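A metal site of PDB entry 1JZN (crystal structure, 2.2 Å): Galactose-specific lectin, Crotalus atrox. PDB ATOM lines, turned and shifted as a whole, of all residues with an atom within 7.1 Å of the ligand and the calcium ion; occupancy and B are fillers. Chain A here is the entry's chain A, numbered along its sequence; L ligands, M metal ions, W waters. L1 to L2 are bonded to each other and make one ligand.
N of His 99 sits at hydrogen-bond distance from OD2 of Asp 120 (2.8 Å).
The side-chain carboxylate (OE2) of Glu 104 lies close to the backbone NH (N) of Tyr 100 (3.3 Å).
N of Glu 108 sits at hydrogen-bond distance from O of Asn 119, 2.9 Å away.
N of Tyr 100 lies close to OD1 of Asp 98 (3.1 Å).
Merely in contact with the ligand: Tyr 100 (3.8 Å).
Hydrophobic or aromatic side chains within 4 Å of the ligand: Tyr 100.
Six residues have an atom within 4 Å of the ligand: Gln 96, Asp 98, Tyr 100, Glu 104, Asn 119 and Asp 120.
Within 4 Å of the calcium ion: Gln 96, Asp 98, Glu 104, Asn 119 and Asp 120.
The nearest printed residue that does not touch the calcium ion is Tyr 100 (4.7 Å).
The calcium ion is bound by the side-chain carboxylate (OD1) of Asp 120 (2.2 Å), the side-chain amide oxygen (OE1) of Gln 96 (2.5 Å), the side-chain carboxylate (OE2) of Glu 104 (2.5 Å), the side-chain amide oxygen (OD1) of Asn 119 (2.5 Å), an oxygen (O3) of LG2 L2 (2.6 Å), the backbone carbonyl oxygen (O) of Asp 120 (2.6 Å), the side-chain carboxylate (OD1) of Asp 98 (2.6 Å) and an oxygen (O2) of LG2 L2 (2.7 Å).
The calcium ion has eight donor atoms within binding distance.
Water W1 lies within hydrogen-bond range of the backbone carbonyl oxygen (O) of Lys 94 (2.6 Å), the side-chain amide nitrogen (NE2) of Gln 96 (3.0 Å), an oxygen (O3) of LIG L1 (3.1 Å) and the side-chain carboxylate (OD2) of Asp 93 (3.5 Å).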
ATOM      1  N   ASN A  65      15.047 -20.625   8.539  1.00  0.00           N
ATOM      2  CA  ASN A  65      13.761 -20.503   7.842  1.00  0.00           C
ATOM      3  C   ASN A  65      13.583 -19.030   7.524  1.00  0.00           C
ATOM      4  O   ASN A  65      14.329 -18.210   8.045  1.00  0.00           O
ATOM      5  CB  ASN A  65      12.631 -21.036   8.705  1.00  0.00           C
ATOM      6  CG  ASN A  65      12.837 -22.481   9.054  1.00  0.00           C
ATOM      7  OD1 ASN A  65      13.222 -23.293   8.200  1.00  0.00           O
ATOM      8  ND2 ASN A  65      12.598 -22.826  10.316  1.00  0.00           N
ATOM      9  N   TRP A  92       0.741 -24.821   2.464  1.00  0.00           N
ATOM     10  CA  TRP A  92       1.174 -25.315   3.766  1.00  0.00           C
ATOM     11  C   TRP A  92       1.978 -26.596   3.691  1.00  0.00           C
ATOM     12  O   TRP A  92       1.744 -27.445   2.834  1.00  0.00           O
ATOM     13  CB  TRP A  92      -0.056 -25.570   4.644  1.00  0.00           C
ATOM     14  CG  TRP A  92      -0.836 -24.331   5.014  1.00  0.00           C
ATOM     15  CD1 TRP A  92      -2.113 -24.020   4.627  1.00  0.00           C
ATOM     16  CD2 TRP A  92      -0.406 -23.277   5.882  1.00  0.00           C
ATOM     17  NE1 TRP A  92      -2.497 -22.824   5.208  1.00  0.00           N
ATOM     18  CE2 TRP A  92      -1.464 -22.358   5.981  1.00  0.00           C
ATOM     19  CE3 TRP A  92       0.782 -23.022   6.590  1.00  0.00           C
ATOM     20  CZ2 TRP A  92      -1.383 -21.207   6.764  1.00  0.00           C
ATOM     21  CZ3 TRP A  92       0.865 -21.891   7.364  1.00  0.00           C
ATOM     22  CH2 TRP A  92      -0.212 -20.992   7.439  1.00  0.00           C
ATOM     23  N   ASP A  93       2.926 -26.751   4.616  1.00  0.00           N
ATOM     24  CA  ASP A  93       3.735 -27.960   4.676  1.00  0.00           C
ATOM     25  C   ASP A  93       2.845 -29.055   5.287  1.00  0.00           C
ATOM     26  O   ASP A  93       1.736 -28.797   5.754  1.00  0.00           O
ATOM     27  CB  ASP A  93       4.975 -27.711   5.546  1.00  0.00           C
ATOM     28  CG  ASP A  93       5.970 -28.858   5.475  1.00  0.00           C
ATOM     29  OD1 ASP A  93       5.743 -29.805   4.685  1.00  0.00           O
ATOM     30  OD2 ASP A  93       6.973 -28.813   6.227  1.00  0.00           O
ATOM     31  N   LYS A  94       3.325 -30.292   5.249  1.00  0.00           N
ATOM     32  CA  LYS A  94       2.587 -31.419   5.791  1.00  0.00           C
ATOM     33  C   LYS A  94       2.094 -31.159   7.231  1.00  0.00           C
ATOM     34  O   LYS A  94       2.875 -30.802   8.117  1.00  0.00           O
ATOM     35  CB  LYS A  94       3.477 -32.649   5.756  1.00  0.00           C
ATOM     36  CG  LYS A  94       2.860 -33.917   6.303  1.00  0.00           C
ATOM     37  CD  LYS A  94       3.912 -35.017   6.364  1.00  0.00           C
ATOM     38  CE  LYS A  94       3.414 -36.266   7.083  1.00  0.00           C
ATOM     39  NZ  LYS A  94       4.501 -37.287   7.173  1.00  0.00           N
ATOM     40  N   ASN A  95       0.796 -31.351   7.434  1.00  0.00           N
ATOM     41  CA  ASN A  95       0.147 -31.166   8.733  1.00  0.00           C
ATOM     42  C   ASN A  95       0.210 -29.769   9.328  1.00  0.00           C
ATOM     43  O   ASN A  95       0.163 -29.589  10.533  1.00  0.00           O
ATOM     44  CB  ASN A  95       0.669 -32.215   9.743  1.00  0.00           C
ATOM     45  CG  ASN A  95       0.259 -33.645   9.362  1.00  0.00           C
ATOM     46  OD1 ASN A  95       1.010 -34.596   9.570  1.00  0.00           O
ATOM     47  ND2 ASN A  95      -0.947 -33.789   8.808  1.00  0.00           N
ATOM     48  N   GLN A  96       0.285 -28.782   8.438  1.00  0.00           N
ATOM     49  CA  GLN A  96       0.306 -27.377   8.857  1.00  0.00           C
ATOM     50  C   GLN A  96      -0.906 -26.744   8.161  1.00  0.00           C
ATOM     51  O   GLN A  96      -1.368 -27.228   7.123  1.00  0.00           O
ATOM     52  CB  GLN A  96       1.588 -26.698   8.412  1.00  0.00           C
ATOM     53  CG  GLN A  96       2.870 -27.338   8.950  1.00  0.00           C
ATOM     54  CD  GLN A  96       2.897 -27.463  10.472  1.00  0.00           C
ATOM     55  OE1 GLN A  96       2.292 -26.667  11.186  1.00  0.00           O
ATOM     56  NE2 GLN A  96       3.624 -28.474  10.973  1.00  0.00           N
ATOM     57  N   PRO A  97      -1.452 -25.667   8.739  1.00  0.00           N
ATOM     58  CA  PRO A  97      -1.011 -25.028   9.985  1.00  0.00           C
ATOM     59  C   PRO A  97      -1.622 -25.790  11.166  1.00  0.00           C
ATOM     60  O   PRO A  97      -2.716 -26.334  11.047  1.00  0.00           O
ATOM     61  CB  PRO A  97      -1.555 -23.614   9.850  1.00  0.00           C
ATOM     62  CG  PRO A  97      -2.866 -23.836   9.147  1.00  0.00           C
ATOM     63  CD  PRO A  97      -2.525 -24.879   8.092  1.00  0.00           C
ATOM     64  N   ASP A  98      -0.942 -25.821  12.299  1.00  0.00           N
ATOM     65  CA  ASP A  98      -1.492 -26.588  13.422  1.00  0.00           C
ATOM     66  C   ASP A  98      -1.632 -25.812  14.732  1.00  0.00           C
ATOM     67  O   ASP A  98      -2.087 -26.388  15.732  1.00  0.00           O
ATOM     68  CB  ASP A  98      -0.620 -27.832  13.656  1.00  0.00           C
ATOM     69  CG  ASP A  98       0.790 -27.461  14.088  1.00  0.00           C
ATOM     70  OD1 ASP A  98       1.124 -26.265  14.048  1.00  0.00           O
ATOM     71  OD2 ASP A  98       1.568 -28.357  14.471  1.00  0.00           O
ATOM     72  N   HIS A  99      -1.262 -24.540  14.749  1.00  0.00           N
ATOM     73  CA  HIS A  99      -1.313 -23.751  15.988  1.00  0.00           C
ATOM     74  C   HIS A  99      -0.726 -24.574  17.141  1.00  0.00           C
ATOM     75  O   HIS A  99      -1.315 -24.671  18.234  1.00  0.00           O
ATOM     76  CB  HIS A  99      -2.744 -23.342  16.353  1.00  0.00           C
ATOM     77  CG  HIS A  99      -3.247 -22.121  15.629  1.00  0.00           C
ATOM     78  ND1 HIS A  99      -4.471 -21.538  15.902  1.00  0.00           N
ATOM     79  CD2 HIS A  99      -2.685 -21.362  14.654  1.00  0.00           C
ATOM     80  CE1 HIS A  99      -4.641 -20.482  15.137  1.00  0.00           C
ATOM     81  NE2 HIS A  99      -3.571 -20.356  14.368  1.00  0.00           N
ATOM     82  N   TYR A 100       0.430 -25.193  16.894  1.00  0.00           N
ATOM     83  CA  TYR A 100       1.086 -26.018  17.897  1.00  0.00           C
ATOM     84  C   TYR A 100       1.142 -25.311  19.247  1.00  0.00           C
ATOM     85  O   TYR A 100       1.643 -24.188  19.354  1.00  0.00           O
ATOM     86  CB  TYR A 100       2.501 -26.353  17.420  1.00  0.00           C
ATOM     87  CG  TYR A 100       3.228 -27.335  18.271  1.00  0.00           C
ATOM     88  CD1 TYR A 100       4.558 -27.118  18.618  1.00  0.00           C
ATOM     89  CD2 TYR A 100       2.612 -28.495  18.730  1.00  0.00           C
ATOM     90  CE1 TYR A 100       5.259 -28.031  19.398  1.00  0.00           C
ATOM     91  CE2 TYR A 100       3.294 -29.417  19.517  1.00  0.00           C
ATOM     92  CZ  TYR A 100       4.622 -29.171  19.853  1.00  0.00           C
ATOM     93  OH  TYR A 100       5.318 -30.010  20.676  1.00  0.00           O
ATOM     94  N   LYS A 103       0.735 -21.257  20.301  1.00  0.00           N
ATOM     95  CA  LYS A 103       1.796 -20.248  20.376  1.00  0.00           C
ATOM     96  C   LYS A 103       2.312 -19.864  18.994  1.00  0.00           C
ATOM     97  O   LYS A 103       3.257 -19.071  18.863  1.00  0.00           O
ATOM     98  CB  LYS A 103       2.972 -20.788  21.188  1.00  0.00           C
ATOM     99  CG  LYS A 103       3.608 -22.017  20.544  1.00  0.00           C
ATOM    100  CD  LYS A 103       4.849 -22.481  21.285  1.00  0.00           C
ATOM    101  CE  LYS A 103       5.446 -23.725  20.626  1.00  0.00           C
ATOM    102  NZ  LYS A 103       6.423 -24.416  21.525  1.00  0.00           N
ATOM    103  N   GLU A 104       1.696 -20.421  17.943  1.00  0.00           N
ATOM    104  CA  GLU A 104       2.112 -20.180  16.569  1.00  0.00           C
ATOM    105  C   GLU A 104       1.137 -19.372  15.717  1.00  0.00           C
ATOM    106  O   GLU A 104       0.090 -19.890  15.308  1.00  0.00           O
ATOM    107  CB  GLU A 104       2.376 -21.517  15.891  1.00  0.00           C
ATOM    108  CG  GLU A 104       3.400 -22.317  16.622  1.00  0.00           C
ATOM    109  CD  GLU A 104       3.789 -23.598  15.905  1.00  0.00           C
ATOM    110  OE1 GLU A 104       4.909 -24.093  16.161  1.00  0.00           O
ATOM    111  OE2 GLU A 104       2.990 -24.116  15.109  1.00  0.00           O
ATOM    112  N   CYS A 106       2.512 -16.791  13.160  1.00  0.00           N
ATOM    113  CA  CYS A 106       3.214 -16.170  12.034  1.00  0.00           C
ATOM    114  C   CYS A 106       3.719 -17.268  11.072  1.00  0.00           C
ATOM    115  O   CYS A 106       4.032 -18.379  11.489  1.00  0.00           O
ATOM    116  CB  CYS A 106       4.366 -15.288  12.578  1.00  0.00           C
ATOM    117  SG  CYS A 106       3.740 -13.906  13.614  1.00  0.00           S
ATOM    118  N   GLU A 108       6.320 -18.913   8.201  1.00  0.00           N
ATOM    119  CA  GLU A 108       7.693 -18.953   7.661  1.00  0.00           C
ATOM    120  C   GLU A 108       7.792 -19.982   6.504  1.00  0.00           C
ATOM    121  O   GLU A 108       6.998 -20.936   6.425  1.00  0.00           O
ATOM    122  CB  GLU A 108       8.691 -19.365   8.773  1.00  0.00           C
ATOM    123  CG  GLU A 108       8.457 -20.803   9.299  1.00  0.00           C
ATOM    124  CD  GLU A 108       9.292 -21.182  10.529  1.00  0.00           C
ATOM    125  OE1 GLU A 108       9.167 -22.336  10.997  1.00  0.00           O
ATOM    126  OE2 GLU A 108      10.077 -20.351  11.030  1.00  0.00           O
ATOM    127  N   VAL A 110       9.694 -22.972   5.013  1.00  0.00           N
ATOM    128  CA  VAL A 110      10.514 -24.006   5.666  1.00  0.00           C
ATOM    129  C   VAL A 110      11.773 -24.423   4.912  1.00  0.00           C
ATOM    130  O   VAL A 110      11.686 -24.966   3.814  1.00  0.00           O
ATOM    131  CB  VAL A 110       9.653 -25.252   5.964  1.00  0.00           C
ATOM    132  CG1 VAL A 110      10.453 -26.286   6.745  1.00  0.00           C
ATOM    133  CG2 VAL A 110       8.413 -24.836   6.746  1.00  0.00           C
ATOM    134  N   LEU A 112      13.888 -26.884   5.299  1.00  0.00           N
ATOM    135  CA  LEU A 112      13.968 -28.309   4.941  1.00  0.00           C
ATOM    136  C   LEU A 112      13.168 -28.697   3.703  1.00  0.00           C
ATOM    137  O   LEU A 112      13.393 -29.771   3.144  1.00  0.00           O
ATOM    138  CB  LEU A 112      13.527 -29.201   6.107  1.00  0.00           C
ATOM    139  CG  LEU A 112      14.652 -29.575   7.079  1.00  0.00           C
ATOM    140  CD1 LEU A 112      14.062 -30.349   8.245  1.00  0.00           C
ATOM    141  CD2 LEU A 112      15.721 -30.407   6.342  1.00  0.00           C
ATOM    142  N   TRP A 118       4.994 -23.802   3.630  1.00  0.00           N
ATOM    143  CA  TRP A 118       4.850 -22.962   4.797  1.00  0.00           C
ATOM    144  C   TRP A 118       4.566 -23.659   6.123  1.00  0.00           C
ATOM    145  O   TRP A 118       4.005 -24.773   6.174  1.00  0.00           O
ATOM    146  CB  TRP A 118       3.742 -21.935   4.573  1.00  0.00           C
ATOM    147  CG  TRP A 118       3.744 -21.223   3.245  1.00  0.00           C
ATOM    148  CD1 TRP A 118       4.799 -21.040   2.404  1.00  0.00           C
ATOM    149  CD2 TRP A 118       2.647 -20.509   2.669  1.00  0.00           C
ATOM    150  NE1 TRP A 118       4.425 -20.240   1.346  1.00  0.00           N
ATOM    151  CE2 TRP A 118       3.109 -19.913   1.487  1.00  0.00           C
ATOM    152  CE3 TRP A 118       1.302 -20.330   3.045  1.00  0.00           C
ATOM    153  CZ2 TRP A 118       2.276 -19.120   0.668  1.00  0.00           C
ATOM    154  CZ3 TRP A 118       0.469 -19.536   2.226  1.00  0.00           C
ATOM    155  CH2 TRP A 118       0.972 -18.946   1.050  1.00  0.00           C
ATOM    156  N   ASN A 119       4.933 -22.972   7.197  1.00  0.00           N
ATOM    157  CA  ASN A 119       4.723 -23.438   8.546  1.00  0.00           C
ATOM    158  C   ASN A 119       4.322 -22.275   9.436  1.00  0.00           C
ATOM    159  O   ASN A 119       4.916 -21.196   9.338  1.00  0.00           O
ATOM    160  CB  ASN A 119       5.994 -24.070   9.142  1.00  0.00           C
ATOM    161  CG  ASN A 119       5.817 -24.426  10.622  1.00  0.00           C
ATOM    162  OD1 ASN A 119       4.821 -25.053  10.976  1.00  0.00           O
ATOM    163  ND2 ASN A 119       6.775 -24.018  11.490  1.00  0.00           N
ATOM    164  N   ASP A 120       3.329 -22.482  10.287  1.00  0.00           N
ATOM    165  CA  ASP A 120       2.959 -21.458  11.241  1.00  0.00           C
ATOM    166  C   ASP A 120       3.951 -21.648  12.404  1.00  0.00           C
ATOM    167  O   ASP A 120       4.184 -22.761  12.857  1.00  0.00           O
ATOM    168  CB  ASP A 120       1.453 -21.535  11.636  1.00  0.00           C
ATOM    169  CG  ASP A 120       1.012 -22.888  12.223  1.00  0.00           C
ATOM    170  OD1 ASP A 120       1.638 -23.938  11.988  1.00  0.00           O
ATOM    171  OD2 ASP A 120      -0.039 -22.869  12.913  1.00  0.00           O
ATOM    172  N   GLN A 121       4.547 -20.555  12.862  1.00  0.00           N
ATOM    173  CA  GLN A 121       5.599 -20.611  13.867  1.00  0.00           C
ATOM    174  C   GLN A 121       5.488 -19.549  14.984  1.00  0.00           C
ATOM    175  O   GLN A 121       4.736 -18.587  14.871  1.00  0.00           O
ATOM    176  CB  GLN A 121       6.926 -20.445  13.107  1.00  0.00           C
ATOM    177  CG  GLN A 121       8.192 -20.417  13.925  1.00  0.00           C
ATOM    178  CD  GLN A 121       8.428 -21.702  14.674  1.00  0.00           C
ATOM    179  OE1 GLN A 121       8.023 -21.842  15.838  1.00  0.00           O
ATOM    180  NE2 GLN A 121       9.076 -22.665  14.022  1.00  0.00           N
ATOM    181  N   VAL A 122       6.249 -19.740  16.058  1.00  0.00           N
ATOM    182  CA  VAL A 122       6.284 -18.764  17.136  1.00  0.00           C
ATOM    183  C   VAL A 122       6.829 -17.457  16.515  1.00  0.00           C
ATOM    184  O   VAL A 122       7.947 -17.430  15.985  1.00  0.00           O
ATOM    185  CB  VAL A 122       7.272 -19.177  18.248  1.00  0.00           C
ATOM    186  CG1 VAL A 122       7.290 -18.097  19.345  1.00  0.00           C
ATOM    187  CG2 VAL A 122       6.881 -20.531  18.813  1.00  0.00           C
HETATM  188  C1  LIG L   1       9.149 -32.499  11.138  1.00  0.00           C
HETATM  189  C2  LIG L   1       8.286 -31.239  11.176  1.00  0.00           C
HETATM  190  C3  LIG L   1       8.564 -30.421  12.435  1.00  0.00           C
HETATM  191  C4  LIG L   1      10.080 -30.162  12.563  1.00  0.00           C
HETATM  192  C5  LIG L   1      10.484 -29.420  13.827  1.00  0.00           C
HETATM  193  C6  LIG L   1      10.614 -32.097  11.302  1.00  0.00           C
HETATM  194  O1  LIG L   1      11.418 -33.231  11.313  1.00  0.00           O
HETATM  195  O2  LIG L   1       8.970 -33.169   9.893  1.00  0.00           O
HETATM  196  O3  LIG L   1       6.908 -31.594  11.108  1.00  0.00           O
HETATM  197  O4  LIG L   1       7.872 -29.172  12.349  1.00  0.00           O
HETATM  198  O5  LIG L   1      10.782 -31.414  12.549  1.00  0.00           O
HETATM  199  O6  LIG L   1      10.268 -30.230  14.978  1.00  0.00           O
HETATM  200  C1  LG2 L   2       7.300 -28.668  13.509  1.00  0.00           C
HETATM  201  C2  LG2 L   2       6.943 -27.202  13.277  1.00  0.00           C
HETATM  202  C3  LG2 L   2       6.156 -26.631  14.461  1.00  0.00           C
HETATM  203  C4  LG2 L   2       4.980 -27.545  14.845  1.00  0.00           C
HETATM  204  C5  LG2 L   2       5.467 -29.002  15.012  1.00  0.00           C
HETATM  205  C6  LG2 L   2       4.336 -29.983  15.311  1.00  0.00           C
HETATM  206  O1  LG2 L   2       8.142 -26.462  13.074  1.00  0.00           O
HETATM  207  O2  LG2 L   2       5.660 -25.347  14.099  1.00  0.00           O
HETATM  208  O3  LG2 L   2       3.979 -27.486  13.840  1.00  0.00           O
HETATM  209  O4  LG2 L   2       6.114 -29.431  13.795  1.00  0.00           O
HETATM  210  O5  LG2 L   2       4.805 -31.156  15.968  1.00  0.00           O
HETATM  211 CA    CA M   1       3.237 -25.199  12.907  1.00  0.00          CA
HETATM  212  O   HOH W   1       5.205 -30.107   8.955  1.00  0.00           O
HETATM  213  O   HOH W   2       2.396 -31.891  16.798  1.00  0.00           O
HETATM  214  O   HOH W   3      12.181 -36.030  11.206  1.00  0.00           O
HETATM  215  O   HOH W   4       5.245 -32.169  13.138  1.00  0.00           O
HETATM  216  O   HOH W   5       8.734 -27.095  10.125  1.00  0.00           O
HETATM  217  O   HOH W   6      13.871 -32.549  10.541  1.00  0.00           O
